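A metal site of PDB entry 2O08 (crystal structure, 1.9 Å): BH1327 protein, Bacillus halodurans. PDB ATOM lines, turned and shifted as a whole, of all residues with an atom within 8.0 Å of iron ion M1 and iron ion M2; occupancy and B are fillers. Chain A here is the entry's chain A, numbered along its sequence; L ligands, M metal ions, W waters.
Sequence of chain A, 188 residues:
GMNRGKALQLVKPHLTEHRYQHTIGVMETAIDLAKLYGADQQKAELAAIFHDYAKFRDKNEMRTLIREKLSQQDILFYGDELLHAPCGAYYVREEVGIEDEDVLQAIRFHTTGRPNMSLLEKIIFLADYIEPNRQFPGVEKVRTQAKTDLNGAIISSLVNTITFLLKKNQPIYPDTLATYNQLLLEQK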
ATOM      1  N   ARG A  19     -32.425  14.526  14.662  1.00  0.00           N
ATOM      2  CA  ARG A  19     -31.049  14.993  14.796  1.00  0.00           C
ATOM      3  C   ARG A  19     -30.082  13.837  15.079  1.00  0.00           C
ATOM      4  O   ARG A  19     -28.929  13.859  14.624  1.00  0.00           O
ATOM      5  CB  ARG A  19     -30.932  16.093  15.866  1.00  0.00           C
ATOM      6  CG  ARG A  19     -31.713  17.378  15.496  1.00  0.00           C
ATOM      7  CD  ARG A  19     -31.379  17.994  14.134  1.00  0.00           C
ATOM      8  NE  ARG A  19     -29.993  18.426  14.027  1.00  0.00           N
ATOM      9  CZ  ARG A  19     -29.481  19.104  12.988  1.00  0.00           C
ATOM     10  NH1 ARG A  19     -30.224  19.506  11.953  1.00  0.00           N
ATOM     11  NH2 ARG A  19     -28.206  19.443  13.004  1.00  0.00           N
ATOM     12  N   HIS A  22     -29.419  12.349  11.763  1.00  0.00           N
ATOM     13  CA  HIS A  22     -28.469  13.225  11.074  1.00  0.00           C
ATOM     14  C   HIS A  22     -27.025  12.937  11.490  1.00  0.00           C
ATOM     15  O   HIS A  22     -26.128  12.837  10.641  1.00  0.00           O
ATOM     16  CB  HIS A  22     -28.805  14.705  11.351  1.00  0.00           C
ATOM     17  CG  HIS A  22     -27.821  15.672  10.770  1.00  0.00           C
ATOM     18  ND1 HIS A  22     -27.584  15.757   9.416  1.00  0.00           N
ATOM     19  CD2 HIS A  22     -27.043  16.609  11.356  1.00  0.00           C
ATOM     20  CE1 HIS A  22     -26.694  16.719   9.188  1.00  0.00           C
ATOM     21  NE2 HIS A  22     -26.346  17.239  10.347  1.00  0.00           N
ATOM     22  N   THR A  23     -26.798  12.778  12.798  1.00  0.00           N
ATOM     23  CA  THR A  23     -25.455  12.592  13.350  1.00  0.00           C
ATOM     24  C   THR A  23     -24.822  11.320  12.849  1.00  0.00           C
ATOM     25  O   THR A  23     -23.671  11.319  12.359  1.00  0.00           O
ATOM     26  CB  THR A  23     -25.516  12.590  14.917  1.00  0.00           C
ATOM     27  OG1 THR A  23     -26.182  13.794  15.343  1.00  0.00           O
ATOM     28  CG2 THR A  23     -24.094  12.503  15.586  1.00  0.00           C
ATOM     29  N   VAL A  26     -24.121  11.638   9.098  1.00  0.00           N
ATOM     30  CA  VAL A  26     -22.857  12.417   8.848  1.00  0.00           C
ATOM     31  C   VAL A  26     -21.609  11.575   9.204  1.00  0.00           C
ATOM     32  O   VAL A  26     -20.596  11.532   8.445  1.00  0.00           O
ATOM     33  CB  VAL A  26     -22.865  13.767   9.586  1.00  0.00           C
ATOM     34  CG1 VAL A  26     -21.544  14.548   9.351  1.00  0.00           C
ATOM     35  CG2 VAL A  26     -24.044  14.578   9.135  1.00  0.00           C
ATOM     36  N   ALA A  48     -17.345  14.348  12.859  1.00  0.00           N
ATOM     37  CA  ALA A  48     -18.753  14.138  12.464  1.00  0.00           C
ATOM     38  C   ALA A  48     -19.711  14.050  13.629  1.00  0.00           C
ATOM     39  O   ALA A  48     -20.727  14.741  13.636  1.00  0.00           O
ATOM     40  CB  ALA A  48     -18.893  12.942  11.598  1.00  0.00           C
ATOM     41  N   HIS A  51     -19.841  17.646  15.036  1.00  0.00           N
ATOM     42  CA  HIS A  51     -19.891  18.841  14.166  1.00  0.00           C
ATOM     43  C   HIS A  51     -21.002  19.865  14.544  1.00  0.00           C
ATOM     44  O   HIS A  51     -20.788  21.082  14.453  1.00  0.00           O
ATOM     45  CB  HIS A  51     -19.958  18.479  12.674  1.00  0.00           C
ATOM     46  CG  HIS A  51     -21.313  18.122  12.190  1.00  0.00           C
ATOM     47  ND1 HIS A  51     -21.906  16.910  12.479  1.00  0.00           N
ATOM     48  CD2 HIS A  51     -22.198  18.807  11.418  1.00  0.00           C
ATOM     49  CE1 HIS A  51     -23.117  16.877  11.933  1.00  0.00           C
ATOM     50  NE2 HIS A  51     -23.306  18.001  11.264  1.00  0.00           N
ATOM     51  N   ASP A  52     -22.129  19.364  15.001  1.00  0.00           N
ATOM     52  CA  ASP A  52     -23.285  20.198  15.361  1.00  0.00           C
ATOM     53  C   ASP A  52     -23.521  20.313  16.853  1.00  0.00           C
ATOM     54  O   ASP A  52     -24.630  20.666  17.290  1.00  0.00           O
ATOM     55  CB  ASP A  52     -24.572  19.698  14.695  1.00  0.00           C
ATOM     56  CG  ASP A  52     -24.707  20.173  13.244  1.00  0.00           C
ATOM     57  OD1 ASP A  52     -24.154  21.188  12.871  1.00  0.00           O
ATOM     58  OD2 ASP A  52     -25.390  19.508  12.474  1.00  0.00           O
ATOM     59  N   TYR A  53     -22.456  20.103  17.623  1.00  0.00           N
ATOM     60  CA  TYR A  53     -22.514  20.228  19.070  1.00  0.00           C
ATOM     61  C   TYR A  53     -23.224  21.484  19.584  1.00  0.00           C
ATOM     62  O   TYR A  53     -23.954  21.413  20.580  1.00  0.00           O
ATOM     63  CB  TYR A  53     -21.098  20.197  19.620  1.00  0.00           C
ATOM     64  CG  TYR A  53     -20.985  20.284  21.099  1.00  0.00           C
ATOM     65  CD1 TYR A  53     -21.246  19.173  21.910  1.00  0.00           C
ATOM     66  CD2 TYR A  53     -20.556  21.470  21.710  1.00  0.00           C
ATOM     67  CE1 TYR A  53     -21.074  19.249  23.316  1.00  0.00           C
ATOM     68  CE2 TYR A  53     -20.372  21.542  23.077  1.00  0.00           C
ATOM     69  CZ  TYR A  53     -20.605  20.432  23.873  1.00  0.00           C
ATOM     70  OH  TYR A  53     -20.440  20.594  25.231  1.00  0.00           O
ATOM     71  N   ALA A  54     -22.963  22.633  18.968  1.00  0.00           N
ATOM     72  CA  ALA A  54     -23.525  23.919  19.428  1.00  0.00           C
ATOM     73  C   ALA A  54     -24.820  24.347  18.691  1.00  0.00           C
ATOM     74  O   ALA A  54     -25.309  25.441  18.892  1.00  0.00           O
ATOM     75  CB  ALA A  54     -22.447  25.011  19.318  1.00  0.00           C
ATOM     76  N   LYS A  55     -25.387  23.481  17.849  1.00  0.00           N
ATOM     77  CA  LYS A  55     -26.551  23.868  17.032  1.00  0.00           C
ATOM     78  C   LYS A  55     -27.657  24.489  17.887  1.00  0.00           C
ATOM     79  O   LYS A  55     -28.235  25.488  17.509  1.00  0.00           O
ATOM     80  CB  LYS A  55     -27.047  22.632  16.281  1.00  0.00           C
ATOM     81  CG  LYS A  55     -28.260  22.790  15.428  1.00  0.00           C
ATOM     82  CD  LYS A  55     -27.988  23.336  14.080  1.00  0.00           C
ATOM     83  CE  LYS A  55     -29.305  23.381  13.314  1.00  0.00           C
ATOM     84  NZ  LYS A  55     -28.968  23.865  11.976  1.00  0.00           N
ATOM     85  N   GLU A  81     -27.351  30.924  11.324  1.00  0.00           N
ATOM     86  CA  GLU A  81     -26.886  29.579  10.996  1.00  0.00           C
ATOM     87  C   GLU A  81     -25.362  29.455  11.021  1.00  0.00           C
ATOM     88  O   GLU A  81     -24.853  28.353  11.153  1.00  0.00           O
ATOM     89  CB  GLU A  81     -27.446  29.106   9.631  1.00  0.00           C
ATOM     90  N   HIS A  84     -23.068  28.283  14.941  1.00  0.00           N
ATOM     91  CA  HIS A  84     -22.823  27.043  15.648  1.00  0.00           C
ATOM     92  C   HIS A  84     -21.538  26.322  15.290  1.00  0.00           C
ATOM     93  O   HIS A  84     -21.005  25.612  16.132  1.00  0.00           O
ATOM     94  CB  HIS A  84     -24.037  26.094  15.540  1.00  0.00           C
ATOM     95  CG  HIS A  84     -24.222  25.468  14.194  1.00  0.00           C
ATOM     96  ND1 HIS A  84     -24.891  26.099  13.167  1.00  0.00           N
ATOM     97  CD2 HIS A  84     -23.901  24.242  13.747  1.00  0.00           C
ATOM     98  CE1 HIS A  84     -24.920  25.299  12.117  1.00  0.00           C
ATOM     99  NE2 HIS A  84     -24.333  24.154  12.445  1.00  0.00           N
ATOM    100  N   ALA A  85     -21.035  26.501  14.066  1.00  0.00           N
ATOM    101  CA  ALA A  85     -19.768  25.841  13.671  1.00  0.00           C
ATOM    102  C   ALA A  85     -18.552  26.371  14.462  1.00  0.00           C
ATOM    103  O   ALA A  85     -17.858  25.591  15.107  1.00  0.00           O
ATOM    104  CB  ALA A  85     -19.525  25.927  12.110  1.00  0.00           C
ATOM    105  N   ILE A 107     -14.829  20.969  12.364  1.00  0.00           N
ATOM    106  CA  ILE A 107     -16.069  21.401  12.959  1.00  0.00           C
ATOM    107  C   ILE A 107     -16.307  22.872  12.606  1.00  0.00           C
ATOM    108  O   ILE A 107     -17.395  23.238  12.195  1.00  0.00           O
ATOM    109  CB  ILE A 107     -16.067  21.197  14.497  1.00  0.00           C
ATOM    110  CG1 ILE A 107     -16.021  19.712  14.842  1.00  0.00           C
ATOM    111  CG2 ILE A 107     -17.315  21.848  15.107  1.00  0.00           C
ATOM    112  CD1 ILE A 107     -15.786  19.401  16.328  1.00  0.00           C
ATOM    113  N   HIS A 110     -17.498  23.728   8.810  1.00  0.00           N
ATOM    114  CA  HIS A 110     -18.395  22.785   8.138  1.00  0.00           C
ATOM    115  C   HIS A 110     -19.603  23.439   7.531  1.00  0.00           C
ATOM    116  O   HIS A 110     -20.266  22.818   6.687  1.00  0.00           O
ATOM    117  CB  HIS A 110     -18.873  21.637   9.066  1.00  0.00           C
ATOM    118  CG  HIS A 110     -20.004  21.999   9.976  1.00  0.00           C
ATOM    119  ND1 HIS A 110     -19.812  22.450  11.275  1.00  0.00           N
ATOM    120  CD2 HIS A 110     -21.338  21.952   9.792  1.00  0.00           C
ATOM    121  CE1 HIS A 110     -21.006  22.660  11.833  1.00  0.00           C
ATOM    122  NE2 HIS A 110     -21.943  22.369  10.945  1.00  0.00           N
ATOM    123  N   THR A 111     -19.972  24.614   8.060  1.00  0.00           N
ATOM    124  CA  THR A 111     -21.144  25.345   7.548  1.00  0.00           C
ATOM    125  C   THR A 111     -20.770  26.284   6.370  1.00  0.00           C
ATOM    126  O   THR A 111     -21.447  26.278   5.364  1.00  0.00           O
ATOM    127  CB  THR A 111     -21.796  26.229   8.610  1.00  0.00           C
ATOM    128  OG1 THR A 111     -22.143  25.431   9.726  1.00  0.00           O
ATOM    129  CG2 THR A 111     -23.047  26.922   8.047  1.00  0.00           C
ATOM    130  N   THR A 112     -19.740  27.111   6.542  1.00  0.00           N
ATOM    131  CA  THR A 112     -19.409  28.111   5.546  1.00  0.00           C
ATOM    132  C   THR A 112     -18.375  27.638   4.515  1.00  0.00           C
ATOM    133  O   THR A 112     -18.381  28.115   3.375  1.00  0.00           O
ATOM    134  CB  THR A 112     -18.846  29.344   6.185  1.00  0.00           C
ATOM    135  OG1 THR A 112     -17.600  29.034   6.837  1.00  0.00           O
ATOM    136  CG2 THR A 112     -19.885  30.000   7.166  1.00  0.00           C
ATOM    137  N   ILE A 124     -15.967  16.616   6.187  1.00  0.00           N
ATOM    138  CA  ILE A 124     -17.050  16.985   7.121  1.00  0.00           C
ATOM    139  C   ILE A 124     -18.045  17.940   6.480  1.00  0.00           C
ATOM    140  O   ILE A 124     -19.263  17.758   6.606  1.00  0.00           O
ATOM    141  CB  ILE A 124     -16.516  17.510   8.488  1.00  0.00           C
ATOM    142  CG1 ILE A 124     -15.667  16.437   9.175  1.00  0.00           C
ATOM    143  CG2 ILE A 124     -17.693  17.946   9.433  1.00  0.00           C
ATOM    144  CD1 ILE A 124     -16.393  15.066   9.437  1.00  0.00           C
ATOM    145  N   PHE A 125     -17.552  18.952   5.771  1.00  0.00           N
ATOM    146  CA  PHE A 125     -18.397  19.849   5.024  1.00  0.00           C
ATOM    147  C   PHE A 125     -19.333  19.071   4.115  1.00  0.00           C
ATOM    148  O   PHE A 125     -20.560  19.255   4.097  1.00  0.00           O
ATOM    149  CB  PHE A 125     -17.524  20.812   4.149  1.00  0.00           C
ATOM    150  CG  PHE A 125     -18.341  21.791   3.359  1.00  0.00           C
ATOM    151  CD1 PHE A 125     -18.908  21.427   2.126  1.00  0.00           C
ATOM    152  CD2 PHE A 125     -18.606  23.070   3.868  1.00  0.00           C
ATOM    153  CE1 PHE A 125     -19.729  22.338   1.437  1.00  0.00           C
ATOM    154  CE2 PHE A 125     -19.392  23.963   3.171  1.00  0.00           C
ATOM    155  CZ  PHE A 125     -19.952  23.601   1.966  1.00  0.00           C
ATOM    156  N   ALA A 127     -19.934  15.729   3.971  1.00  0.00           N
ATOM    157  CA  ALA A 127     -20.693  14.659   4.671  1.00  0.00           C
ATOM    158  C   ALA A 127     -21.990  15.222   5.242  1.00  0.00           C
ATOM    159  O   ALA A 127     -23.026  14.614   5.172  1.00  0.00           O
ATOM    160  CB  ALA A 127     -19.816  14.031   5.748  1.00  0.00           C
ATOM    161  N   ASP A 128     -21.932  16.451   5.732  1.00  0.00           N
ATOM    162  CA  ASP A 128     -23.093  17.150   6.279  1.00  0.00           C
ATOM    163  C   ASP A 128     -24.145  17.379   5.227  1.00  0.00           C
ATOM    164  O   ASP A 128     -25.320  17.269   5.468  1.00  0.00           O
ATOM    165  CB  ASP A 128     -22.669  18.512   6.790  1.00  0.00           C
ATOM    166  CG  ASP A 128     -23.776  19.213   7.573  1.00  0.00           C
ATOM    167  OD1 ASP A 128     -24.501  18.560   8.342  1.00  0.00           O
ATOM    168  OD2 ASP A 128     -23.988  20.412   7.409  1.00  0.00           O
ATOM    169  N   TYR A 129     -23.671  17.675   4.022  1.00  0.00           N
ATOM    170  CA  TYR A 129     -24.528  18.006   2.927  1.00  0.00           C
ATOM    171  C   TYR A 129     -25.169  16.801   2.269  1.00  0.00           C
ATOM    172  O   TYR A 129     -26.347  16.866   1.911  1.00  0.00           O
ATOM    173  CB  TYR A 129     -23.683  18.792   1.919  1.00  0.00           C
ATOM    174  CG  TYR A 129     -24.514  19.478   0.914  1.00  0.00           C
ATOM    175  CD1 TYR A 129     -25.061  20.739   1.167  1.00  0.00           C
ATOM    176  CD2 TYR A 129     -24.759  18.863  -0.286  1.00  0.00           C
ATOM    177  CE1 TYR A 129     -25.836  21.368   0.225  1.00  0.00           C
ATOM    178  CE2 TYR A 129     -25.481  19.472  -1.218  1.00  0.00           C
ATOM    179  CZ  TYR A 129     -26.046  20.713  -0.973  1.00  0.00           C
ATOM    180  OH  TYR A 129     -26.797  21.253  -1.966  1.00  0.00           O
ATOM    181  N   GLU A 131     -25.311  13.481   3.572  1.00  0.00           N
ATOM    182  CA  GLU A 131     -25.680  12.329   4.421  1.00  0.00           C
ATOM    183  C   GLU A 131     -27.076  11.842   4.001  1.00  0.00           C
ATOM    184  O   GLU A 131     -27.891  12.652   3.538  1.00  0.00           O
ATOM    185  CB  GLU A 131     -25.582  12.663   5.914  1.00  0.00           C
ATOM    186  CG  GLU A 131     -26.569  13.688   6.429  1.00  0.00           C
ATOM    187  CD  GLU A 131     -27.851  13.133   7.010  1.00  0.00           C
ATOM    188  OE1 GLU A 131     -28.125  11.921   6.888  1.00  0.00           O
ATOM    189  OE2 GLU A 131     -28.599  13.950   7.612  1.00  0.00           O
ATOM    190  N   ARG A 134     -30.611  13.716   4.080  1.00  0.00           N
ATOM    191  CA  ARG A 134     -30.779  15.016   3.444  1.00  0.00           C
ATOM    192  C   ARG A 134     -31.530  14.862   2.125  1.00  0.00           C
ATOM    193  O   ARG A 134     -31.228  13.970   1.350  1.00  0.00           O
ATOM    194  CB  ARG A 134     -29.437  15.656   3.171  1.00  0.00           C
ATOM    195  CG  ARG A 134     -28.658  16.011   4.379  1.00  0.00           C
ATOM    196  CD  ARG A 134     -29.286  17.144   5.175  1.00  0.00           C
ATOM    197  NE  ARG A 134     -28.207  17.994   5.662  1.00  0.00           N
ATOM    198  CZ  ARG A 134     -28.188  18.688   6.795  1.00  0.00           C
ATOM    199  NH1 ARG A 134     -29.185  18.647   7.674  1.00  0.00           N
ATOM    200  NH2 ARG A 134     -27.114  19.411   7.052  1.00  0.00           N
HETATM  201  P1  LIG L   1     -27.264  21.511  10.073  1.00  0.00           P
HETATM  202  O1  LIG L   1     -28.672  21.619  10.568  1.00  0.00           O
HETATM  203  O2  LIG L   1     -26.288  22.301  10.941  1.00  0.00           O
HETATM  204  O3  LIG L   1     -26.864  20.036  10.071  1.00  0.00           O
HETATM  205  O4  LIG L   1     -27.395  22.046   8.660  1.00  0.00           O
HETATM  206 FE    FE M   1     -25.055  18.964  10.405  1.00  0.00          FE
HETATM  207 FE    FE M   2     -24.181  22.382  11.110  1.00  0.00          FE
HETATM  208  O   HOH W   1     -24.058  23.798   9.308  1.00  0.00           O
HETATM  209  O   HOH W   2     -24.472  20.653  10.016  1.00  0.00           O
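OD2 of Asp 52 sits close to NH2 of Arg 19, at 2.9 Å.
The side-chain carboxylate of Glu 131 is in hydrogen-bond range of a ring nitrogen (ND1) of His 22, 2.7 Å away.
The guanidinium group (NH2) of Arg 134 is in salt-bridge range of the side-chain carboxylate (OD2) of Asp 128.
O of Ala 48 lies within hydrogen-bond range of ND1 of His 51 (2.7 Å).
A ring nitrogen (ND1) of His 84 lies within hydrogen-bond range of the backbone carbonyl oxygen of Glu 81 (3.0 Å).
NE2 of His 110 lies close to OG1 of Thr 111 (3.3 Å).
The backbone carbonyl oxygen of Ile 107 is in hydrogen-bond range of a ring nitrogen (ND1) of His 110.
Arg 134 touches iron ion M1 (NH2 to FE, 3.96 Å).
Of the 24 residues printed, 5 come within 4 Å of iron ion M1.
The nearest printed residue that does not touch iron ion M1 is Arg 19 (4.1 Å).
Thr 111 touches iron ion M2 (OG1 to FE, 3.9 Å).
Four residues have an atom within 4 Å of iron ion M2: Asp 52, His 84, His 110 and Thr 111.
The nearest printed residue that does not touch iron ion M2 is His 51 (4.1 Å).
Iron ion M1 is bound by water W2 (1.8 Å), O3 of the ligand (2.1 Å), NE2 of His 22 (2.2 Å), OD2 of Asp 52 (2.2 Å), OD1 of Asp 128 (2.2 Å) and NE2 of His 51 (2.2 Å).
Iron ion M2 is bound by water W2, an oxygen (O2) of the ligand, the side-chain carboxylate (OD1) of Asp 52, a ring nitrogen (NE2) of His 84, a ring nitrogen (NE2) of His 110 and water W1.
Iron ion M2 has six donor atoms within binding distance.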
